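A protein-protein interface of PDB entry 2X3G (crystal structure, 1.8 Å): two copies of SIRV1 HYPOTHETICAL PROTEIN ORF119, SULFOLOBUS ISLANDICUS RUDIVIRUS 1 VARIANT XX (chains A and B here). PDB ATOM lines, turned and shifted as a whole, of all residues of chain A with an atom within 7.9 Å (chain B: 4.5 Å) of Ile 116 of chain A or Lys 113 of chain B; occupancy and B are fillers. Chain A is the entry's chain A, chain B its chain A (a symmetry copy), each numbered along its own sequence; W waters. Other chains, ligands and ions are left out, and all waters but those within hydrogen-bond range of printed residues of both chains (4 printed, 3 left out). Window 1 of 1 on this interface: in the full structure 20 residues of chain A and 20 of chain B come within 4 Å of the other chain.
Printed residues of chain B within 4 Å of Lys 114 of chain A: Lys 113 (2.8 Å).
Of the printed residues of chain B, Ile 116 of chain A touches Asp 2 (3.5 Å), Phe 51 (3.7 Å), Ser 52 (3.5 Å), Ile 53 (3.6 Å), Leu 110 (3.6 Å) and Lys 113 (3.98 Å).
Of the printed residues of chain A, Lys 113 of chain B touches Thr 112, Lys 113, Lys 114 and Ile 116.
Printed residues of chain A within 4 Å of Lys 114 of chain B: Lys 113 (2.8 Å).
The nearest printed residue of chain A that does not touch Lys 113 of chain B is Asp 115 of chain A (4.4 Å).
Water W4 lies within hydrogen-bond range of the side-chain hydroxyl of Ser 52 of chain B and the backbone carbonyl oxygen of Asp 115 of chain A.
Water W3 lies within hydrogen-bond range of the backbone carbonyl oxygen of Lys 111 of chain B, the side-chain amino group of Lys 113 of chain A, the backbone NH of Lys 114 of chain B and the backbone carbonyl oxygen of Thr 112 of chain B.
Water W2 lies within hydrogen-bond range of the side-chain hydroxyl of Thr 112 of chain B, the backbone carbonyl oxygen of Thr 112 of chain A and the side-chain amino group of Lys 113 of chain B.
Water W1 lies within hydrogen-bond range of the side-chain hydroxyl (OG1) of Thr 112 of chain A (2.8 Å), the backbone carbonyl oxygen (O) of Thr 112 of chain B (2.9 Å), the backbone NH (N) of Thr 56 of chain A (2.9 Å) and the side-chain amino group (NZ) of Lys 113 of chain A (3.1 Å).
Among the printed residues, merely in contact across the chains: Asp 115 of chain A with Ile 53 of chain B (3.4 Å), Lys 117 of chain A with Phe 51 of chain B (3.4 Å), Thr 56 of chain A with Thr 112 of chain B (3.4 Å), Ile 116 of chain A with Ser 52 of chain B (3.5 Å), Ile 116 of chain A with Asp 2 of chain B (3.5 Å), Asp 115 of chain A with Ser 52 of chain B (3.6 Å), Ile 116 of chain A with Leu 110 of chain B (3.6 Å), Leu 110 of chain A with Ile 116 of chain B (3.6 Å), Ile 116 of chain A with Ile 53 of chain B (3.6 Å), Ile 53 of chain A with Ile 116 of chain B (3.6 Å), Ile 116 of chain A with Phe 51 of chain B (3.7 Å), Met 118 of chain A with Phe 51 of chain B (3.7 Å), Lys 113 of chain A with Lys 113 of chain B (3.8 Å), Thr 112 of chain A with Thr 112 of chain B (3.9 Å), Ile 116 of chain A with Lys 113 of chain B (3.98 Å) and Lys 113 of chain A with Ile 116 of chain B (3.98 Å).
The backbone carbonyl oxygen (O) of Lys 54 of chain B sits at hydrogen-bond distance from the side-chain amino group (NZ) of Lys 113 of chain B, at 2.7 Å.
The backbone carbonyl oxygen of Lys 54 of chain A sits at hydrogen-bond distance from the side-chain amino group of Lys 113 of chain A (2.7 Å).
Printed residues of chain B that touch a printed residue of chain A: Asp 2, Phe 51, Ser 52, Ile 53, Lys 54, Leu 110, Thr 112, Lys 113, Lys 114 and Ile 116.
Hydrophobic or aromatic side chains of chain B that line the printed part of chain A: Phe 51, Ile 53, Leu 110 and Ile 116.
Of the 13 printed residues of chain A, 10 touch a printed residue of chain B.
Among the printed residues, no Asp or Glu carboxylate lies within 4 Å of a Lys or Arg side-chain nitrogen of the other chain.
The side-chain amino group of Lys 113 of chain B lies within hydrogen-bond range of the backbone carbonyl oxygen of Thr 112 of chain A, 2.9 Å away.
O of Lys 114 of chain B lies within hydrogen-bond range of NZ of Lys 113 of chain A (2.8 Å).
The backbone carbonyl oxygen (O) of Thr 112 of chain B sits at hydrogen-bond distance from the side-chain amino group (NZ) of Lys 113 of chain A, at 2.9 Å.
The backbone carbonyl oxygen (O) of Lys 117 of chain A lies within hydrogen-bond range of the backbone NH (N) of Ser 52 of chain B (2.9 Å).
The backbone NH (N) of Lys 54 of chain B sits at hydrogen-bond distance from the backbone carbonyl oxygen (O) of Asp 115 of chain A (3.1 Å).
NZ of Lys 113 of chain B is in hydrogen-bond range of O of Lys 114 of chain A (2.8 Å).
Leu 110 of chain A touches Ile 116 of chain B, and with the chains exchanged Ile 116 of chain A touches Leu 110 of chain B.
Thr 112 of chain A touches its own counterpart, Thr 112 of chain B.
Thr 112 of chain A touches Lys 113 of chain B, and with the chains exchanged Lys 113 of chain A touches Thr 112 of chain B.
Lys 113 of chain A touches its own counterpart, Lys 113 of chain B.
8 positions are printed for both chains.
Of the 22 pairs that touch across the chains among the printed residues, 12 have their exchanged pair printed and touching as well.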
ATOM      1  N   ILE A  53      20.228  11.252  29.141  1.00  0.00           N
ATOM      2  CA  ILE A  53      19.466  10.248  28.412  1.00  0.00           C
ATOM      3  C   ILE A  53      18.688  10.958  27.311  1.00  0.00           C
ATOM      4  O   ILE A  53      18.040  11.968  27.573  1.00  0.00           O
ATOM      5  CB  ILE A  53      18.432   9.550  29.334  1.00  0.00           C
ATOM      6  CG1 ILE A  53      19.109   8.967  30.577  1.00  0.00           C
ATOM      7  CG2 ILE A  53      17.681   8.460  28.571  1.00  0.00           C
ATOM      8  CD1 ILE A  53      20.021   7.833  30.269  1.00  0.00           C
ATOM      9  N   LYS A  54      18.781  10.458  26.083  1.00  0.00           N
ATOM     10  CA  LYS A  54      17.861  10.856  25.011  1.00  0.00           C
ATOM     11  C   LYS A  54      16.885   9.702  24.817  1.00  0.00           C
ATOM     12  O   LYS A  54      17.309   8.567  24.559  1.00  0.00           O
ATOM     13  CB  LYS A  54      18.613  11.151  23.703  1.00  0.00           C
ATOM     14  CG  LYS A  54      17.725  11.350  22.465  1.00  0.00           C
ATOM     15  CD  LYS A  54      18.543  11.292  21.173  1.00  0.00           C
ATOM     16  CE  LYS A  54      17.694  11.468  19.926  1.00  0.00           C
ATOM     17  NZ  LYS A  54      17.540  10.213  19.126  1.00  0.00           N
ATOM     18  N   THR A  56      14.097   8.032  22.552  1.00  0.00           N
ATOM     19  CA  THR A  56      13.556   8.003  21.194  1.00  0.00           C
ATOM     20  C   THR A  56      12.387   7.029  21.116  1.00  0.00           C
ATOM     21  O   THR A  56      12.579   5.819  21.094  1.00  0.00           O
ATOM     22  CB  THR A  56      14.627   7.621  20.142  1.00  0.00           C
ATOM     23  OG1 THR A  56      14.005   7.438  18.859  1.00  0.00           O
ATOM     24  CG2 THR A  56      15.351   6.343  20.519  1.00  0.00           C
ATOM     25  N   LEU A 110      15.752   5.779  32.979  1.00  0.00           N
ATOM     26  CA  LEU A 110      16.141   4.603  32.187  1.00  0.00           C
ATOM     27  C   LEU A 110      14.964   3.743  31.719  1.00  0.00           C
ATOM     28  O   LEU A 110      15.169   2.665  31.154  1.00  0.00           O
ATOM     29  CB  LEU A 110      17.123   3.730  32.968  1.00  0.00           C
ATOM     30  CG  LEU A 110      18.591   4.136  32.809  1.00  0.00           C
ATOM     31  CD1 LEU A 110      19.394   3.371  33.785  1.00  0.00           C
ATOM     32  CD2 LEU A 110      19.106   3.859  31.414  1.00  0.00           C
ATOM     33  N   LYS A 111      13.737   4.222  31.909  1.00  0.00           N
ATOM     34  CA  LYS A 111      12.568   3.375  31.671  1.00  0.00           C
ATOM     35  C   LYS A 111      12.423   2.936  30.206  1.00  0.00           C
ATOM     36  O   LYS A 111      11.886   1.864  29.936  1.00  0.00           O
ATOM     37  CB  LYS A 111      11.285   4.059  32.171  1.00  0.00           C
ATOM     38  CG  LYS A 111      10.773   5.174  31.292  1.00  0.00           C
ATOM     39  CD  LYS A 111       9.751   6.043  32.047  1.00  0.00           C
ATOM     40  CE  LYS A 111       9.546   7.383  31.381  1.00  0.00           C
ATOM     41  NZ  LYS A 111      10.785   8.256  31.310  1.00  0.00           N
ATOM     42  N   THR A 112      12.882   3.753  29.258  1.00  0.00           N
ATOM     43  CA  THR A 112      12.784   3.378  27.840  1.00  0.00           C
ATOM     44  C   THR A 112      14.006   2.584  27.364  1.00  0.00           C
ATOM     45  O   THR A 112      14.064   2.188  26.201  1.00  0.00           O
ATOM     46  CB  THR A 112      12.616   4.606  26.905  1.00  0.00           C
ATOM     47  OG1 THR A 112      13.831   5.352  26.879  1.00  0.00           O
ATOM     48  CG2 THR A 112      11.449   5.512  27.340  1.00  0.00           C
ATOM     49  N   LYS A 113      14.958   2.345  28.269  1.00  0.00           N
ATOM     50  CA  LYS A 113      16.253   1.756  27.926  1.00  0.00           C
ATOM     51  C   LYS A 113      16.407   0.315  28.422  1.00  0.00           C
ATOM     52  O   LYS A 113      17.493  -0.267  28.338  1.00  0.00           O
ATOM     53  CB  LYS A 113      17.366   2.642  28.493  1.00  0.00           C
ATOM     54  CG  LYS A 113      17.305   4.105  28.057  1.00  0.00           C
ATOM     55  CD  LYS A 113      17.493   4.276  26.571  1.00  0.00           C
ATOM     56  CE  LYS A 113      17.505   5.747  26.132  1.00  0.00           C
ATOM     57  NZ  LYS A 113      17.581   5.857  24.651  1.00  0.00           N
ATOM     58  N   LYS A 114      15.315  -0.265  28.912  1.00  0.00           N
ATOM     59  CA  LYS A 114      15.347  -1.598  29.491  1.00  0.00           C
ATOM     60  C   LYS A 114      14.681  -2.548  28.497  1.00  0.00           C
ATOM     61  O   LYS A 114      14.694  -2.298  27.299  1.00  0.00           O
ATOM     62  CB  LYS A 114      14.631  -1.601  30.851  1.00  0.00           C
ATOM     63  CG  LYS A 114      15.341  -0.805  31.942  1.00  0.00           C
ATOM     64  CD  LYS A 114      14.598  -0.971  33.255  1.00  0.00           C
ATOM     65  CE  LYS A 114      14.950  -2.283  33.962  1.00  0.00           C
ATOM     66  NZ  LYS A 114      16.307  -2.235  34.569  1.00  0.00           N
ATOM     67  N   ASP A 115      14.102  -3.629  29.006  1.00  0.00           N
ATOM     68  CA  ASP A 115      13.377  -4.591  28.188  1.00  0.00           C
ATOM     69  C   ASP A 115      14.275  -5.191  27.117  1.00  0.00           C
ATOM     70  O   ASP A 115      13.858  -5.397  25.983  1.00  0.00           O
ATOM     71  CB  ASP A 115      12.124  -3.972  27.574  1.00  0.00           C
ATOM     72  CG  ASP A 115      11.189  -3.384  28.612  1.00  0.00           C
ATOM     73  OD1 ASP A 115      10.690  -4.129  29.474  1.00  0.00           O
ATOM     74  OD2 ASP A 115      10.926  -2.178  28.549  1.00  0.00           O
ATOM     75  N   ILE A 116      15.506  -5.487  27.521  1.00  0.00           N
ATOM     76  CA  ILE A 116      16.471  -6.223  26.716  1.00  0.00           C
ATOM     77  C   ILE A 116      16.730  -7.551  27.432  1.00  0.00           C
ATOM     78  O   ILE A 116      17.157  -7.555  28.590  1.00  0.00           O
ATOM     79  CB  ILE A 116      17.799  -5.456  26.608  1.00  0.00           C
ATOM     80  CG1 ILE A 116      17.592  -4.071  25.982  1.00  0.00           C
ATOM     81  CG2 ILE A 116      18.806  -6.249  25.794  1.00  0.00           C
ATOM     82  CD1 ILE A 116      18.776  -3.138  26.187  1.00  0.00           C
ATOM     83  N   LYS A 117      16.486  -8.673  26.755  1.00  0.00           N
ATOM     84  CA  LYS A 117      16.559  -9.980  27.410  1.00  0.00           C
ATOM     85  C   LYS A 117      17.166 -11.006  26.468  1.00  0.00           C
ATOM     86  O   LYS A 117      16.767 -11.102  25.324  1.00  0.00           O
ATOM     87  CB  LYS A 117      15.167 -10.420  27.859  1.00  0.00           C
ATOM     88  CG  LYS A 117      15.114 -11.725  28.675  1.00  0.00           C
ATOM     89  CD  LYS A 117      15.977 -11.676  29.922  1.00  0.00           C
ATOM     90  CE  LYS A 117      15.472 -12.623  31.024  1.00  0.00           C
ATOM     91  NZ  LYS A 117      16.541 -12.846  32.082  1.00  0.00           N
ATOM     92  N   MET A 118      18.166 -11.733  26.951  1.00  0.00           N
ATOM     93  CA  MET A 118      18.728 -12.858  26.215  1.00  0.00           C
ATOM     94  C   MET A 118      18.482 -14.110  27.019  1.00  0.00           C
ATOM     95  O   MET A 118      18.860 -14.172  28.195  1.00  0.00           O
ATOM     96  CB  MET A 118      20.226 -12.692  26.003  1.00  0.00           C
ATOM     97  CG  MET A 118      20.921 -13.920  25.377  1.00  0.00           C
ATOM     98  SD  MET A 118      20.458 -14.195  23.499  1.00  0.00           S
ATOM     99  CE  MET A 118      21.740 -12.928  22.712  1.00  0.00           C
ATOM    100  N   SER A 119      17.866 -15.101  26.378  1.00  0.00           N
ATOM    101  CA  SER A 119      17.771 -16.447  26.919  1.00  0.00           C
ATOM    102  C   SER A 119      18.503 -17.421  26.006  1.00  0.00           C
ATOM    103  O   SER A 119      18.602 -17.221  24.807  1.00  0.00           O
ATOM    104  CB  SER A 119      16.305 -16.869  27.069  1.00  0.00           C
ATOM    105  OG  SER A 119      15.697 -17.117  25.814  1.00  0.00           O
ATOM    106  OXT SER A 119      19.015 -18.447  26.438  1.00  0.00           O
ATOM    107  N   ASP B   2      25.971  -8.606  25.081  1.00  0.00           N
ATOM    108  CA  ASP B   2      24.866  -9.168  24.336  1.00  0.00           C
ATOM    109  C   ASP B   2      25.358  -9.427  22.904  1.00  0.00           C
ATOM    110  O   ASP B   2      25.063 -10.459  22.325  1.00  0.00           O
ATOM    111  CB  ASP B   2      23.645  -8.233  24.330  1.00  0.00           C
ATOM    112  CG  ASP B   2      22.770  -8.378  25.581  1.00  0.00           C
ATOM    113  OD1 ASP B   2      22.685  -9.495  26.145  1.00  0.00           O
ATOM    114  OD2 ASP B   2      22.147  -7.371  25.983  1.00  0.00           O
ATOM    115  N   PHE B  51      16.754 -13.573  21.750  1.00  0.00           N
ATOM    116  CA  PHE B  51      17.142 -12.233  22.155  1.00  0.00           C
ATOM    117  C   PHE B  51      15.969 -11.333  21.807  1.00  0.00           C
ATOM    118  O   PHE B  51      15.458 -11.416  20.702  1.00  0.00           O
ATOM    119  CB  PHE B  51      18.394 -11.818  21.398  1.00  0.00           C
ATOM    120  CG  PHE B  51      18.930 -10.482  21.786  1.00  0.00           C
ATOM    121  CD1 PHE B  51      19.234 -10.197  23.113  1.00  0.00           C
ATOM    122  CD2 PHE B  51      19.197  -9.524  20.827  1.00  0.00           C
ATOM    123  CE1 PHE B  51      19.732  -8.965  23.472  1.00  0.00           C
ATOM    124  CE2 PHE B  51      19.716  -8.295  21.177  1.00  0.00           C
ATOM    125  CZ  PHE B  51      19.979  -8.007  22.503  1.00  0.00           C
ATOM    126  N   SER B  52      15.524 -10.520  22.760  1.00  0.00           N
ATOM    127  CA  SER B  52      14.305  -9.748  22.582  1.00  0.00           C
ATOM    128  C   SER B  52      14.487  -8.329  23.054  1.00  0.00           C
ATOM    129  O   SER B  52      15.222  -8.075  24.013  1.00  0.00           O
ATOM    130  CB  SER B  52      13.141 -10.401  23.340  1.00  0.00           C
ATOM    131  OG  SER B  52      13.278 -10.271  24.757  1.00  0.00           O
ATOM    132  N   ILE B  53      13.804  -7.415  22.355  1.00  0.00           N
ATOM    133  CA  ILE B  53      13.789  -5.994  22.671  1.00  0.00           C
ATOM    134  C   ILE B  53      12.347  -5.509  22.589  1.00  0.00           C
ATOM    135  O   ILE B  53      11.658  -5.800  21.613  1.00  0.00           O
ATOM    136  CB  ILE B  53      14.611  -5.182  21.635  1.00  0.00           C
ATOM    137  CG1 ILE B  53      16.035  -5.728  21.512  1.00  0.00           C
ATOM    138  CG2 ILE B  53      14.635  -3.701  22.011  1.00  0.00           C
ATOM    139  CD1 ILE B  53      16.849  -5.522  22.741  1.00  0.00           C
ATOM    140  N   LYS B  54      11.882  -4.809  23.618  1.00  0.00           N
ATOM    141  CA  LYS B  54      10.635  -4.041  23.535  1.00  0.00           C
ATOM    142  C   LYS B  54      11.027  -2.574  23.418  1.00  0.00           C
ATOM    143  O   LYS B  54      11.743  -2.052  24.284  1.00  0.00           O
ATOM    144  CB  LYS B  54       9.750  -4.266  24.773  1.00  0.00           C
ATOM    145  CG  LYS B  54       8.535  -3.333  24.890  1.00  0.00           C
ATOM    146  CD  LYS B  54       7.921  -3.385  26.290  1.00  0.00           C
ATOM    147  CE  LYS B  54       6.725  -2.461  26.448  1.00  0.00           C
ATOM    148  NZ  LYS B  54       7.000  -1.271  27.312  1.00  0.00           N
ATOM    149  N   GLU B  55      10.569  -1.919  22.349  1.00  0.00           N
ATOM    150  CA  GLU B  55      10.810  -0.493  22.143  1.00  0.00           C
ATOM    151  C   GLU B  55       9.629   0.282  22.666  1.00  0.00           C
ATOM    152  O   GLU B  55       8.509   0.041  22.233  1.00  0.00           O
ATOM    153  CB  GLU B  55      10.973  -0.154  20.659  1.00  0.00           C
ATOM    154  CG  GLU B  55      12.172  -0.778  19.994  1.00  0.00           C
ATOM    155  CD  GLU B  55      12.488  -0.152  18.649  1.00  0.00           C
ATOM    156  OE1 GLU B  55      11.588   0.497  18.061  1.00  0.00           O
ATOM    157  OE2 GLU B  55      13.638  -0.304  18.180  1.00  0.00           O
ATOM    158  N   LEU B 110      18.932  -2.293  18.865  1.00  0.00           N
ATOM    159  CA  LEU B 110      19.305  -1.527  20.063  1.00  0.00           C
ATOM    160  C   LEU B 110      19.257  -0.008  19.879  1.00  0.00           C
ATOM    161  O   LEU B 110      19.667   0.740  20.771  1.00  0.00           O
ATOM    162  CB  LEU B 110      20.697  -1.931  20.547  1.00  0.00           C
ATOM    163  CG  LEU B 110      20.710  -3.134  21.496  1.00  0.00           C
ATOM    164  CD1 LEU B 110      22.112  -3.555  21.695  1.00  0.00           C
ATOM    165  CD2 LEU B 110      20.094  -2.802  22.837  1.00  0.00           C
ATOM    166  N   LYS B 111      18.725   0.458  18.751  1.00  0.00           N
ATOM    167  CA  LYS B 111      18.826   1.881  18.420  1.00  0.00           C
ATOM    168  C   LYS B 111      18.095   2.791  19.418  1.00  0.00           C
ATOM    169  O   LYS B 111      18.499   3.934  19.617  1.00  0.00           O
ATOM    170  CB  LYS B 111      18.349   2.143  16.982  1.00  0.00           C
ATOM    171  CG  LYS B 111      16.853   2.109  16.791  1.00  0.00           C
ATOM    172  CD  LYS B 111      16.493   1.983  15.299  1.00  0.00           C
ATOM    173  CE  LYS B 111      15.070   1.519  15.098  1.00  0.00           C
ATOM    174  NZ  LYS B 111      14.761   0.145  15.664  1.00  0.00           N
ATOM    175  N   THR B 112      17.019   2.306  20.036  1.00  0.00           N
ATOM    176  CA  THR B 112      16.288   3.127  21.013  1.00  0.00           C
ATOM    177  C   THR B 112      16.840   2.967  22.435  1.00  0.00           C
ATOM    178  O   THR B 112      16.337   3.601  23.361  1.00  0.00           O
ATOM    179  CB  THR B 112      14.769   2.807  21.049  1.00  0.00           C
ATOM    180  OG1 THR B 112      14.571   1.513  21.617  1.00  0.00           O
ATOM    181  CG2 THR B 112      14.128   2.873  19.650  1.00  0.00           C
ATOM    182  N   LYS B 113      17.873   2.137  22.588  1.00  0.00           N
ATOM    183  CA  LYS B 113      18.395   1.749  23.899  1.00  0.00           C
ATOM    184  C   LYS B 113      19.758   2.374  24.212  1.00  0.00           C
ATOM    185  O   LYS B 113      20.394   2.030  25.213  1.00  0.00           O
ATOM    186  CB  LYS B 113      18.475   0.221  23.968  1.00  0.00           C
ATOM    187  CG  LYS B 113      17.163  -0.503  23.672  1.00  0.00           C
ATOM    188  CD  LYS B 113      16.091  -0.198  24.687  1.00  0.00           C
ATOM    189  CE  LYS B 113      14.791  -0.976  24.440  1.00  0.00           C
ATOM    190  NZ  LYS B 113      13.732  -0.558  25.397  1.00  0.00           N
ATOM    191  N   LYS B 114      20.191   3.309  23.371  1.00  0.00           N
ATOM    192  CA  LYS B 114      21.503   3.918  23.508  1.00  0.00           C
ATOM    193  C   LYS B 114      21.299   5.337  24.038  1.00  0.00           C
ATOM    194  O   LYS B 114      20.320   5.607  24.721  1.00  0.00           O
ATOM    195  CB  LYS B 114      22.232   3.914  22.155  1.00  0.00           C
ATOM    196  CG  LYS B 114      22.620   2.528  21.648  1.00  0.00           C
ATOM    197  CD  LYS B 114      23.421   2.663  20.367  1.00  0.00           C
ATOM    198  CE  LYS B 114      24.893   2.994  20.632  1.00  0.00           C
ATOM    199  NZ  LYS B 114      25.640   1.815  21.146  1.00  0.00           N
ATOM    200  N   ILE B 116      22.871   6.987  26.292  1.00  0.00           N
ATOM    201  CA  ILE B 116      23.090   7.085  27.728  1.00  0.00           C
ATOM    202  C   ILE B 116      24.554   7.487  27.929  1.00  0.00           C
ATOM    203  O   ILE B 116      25.457   6.776  27.480  1.00  0.00           O
ATOM    204  CB  ILE B 116      22.853   5.732  28.417  1.00  0.00           C
ATOM    205  CG1 ILE B 116      21.426   5.226  28.172  1.00  0.00           C
ATOM    206  CG2 ILE B 116      23.117   5.841  29.908  1.00  0.00           C
ATOM    207  CD1 ILE B 116      21.248   3.751  28.503  1.00  0.00           C
HETATM  208  O   HOH W   1      14.500   5.645  24.182  1.00  0.00           O
HETATM  209  O   HOH W   2      12.724   1.853  23.687  1.00  0.00           O
HETATM  210  O   HOH W   3      18.669   5.565  21.831  1.00  0.00           O
HETATM  211  O   HOH W   4      12.819  -8.225  26.054  1.00  0.00           O
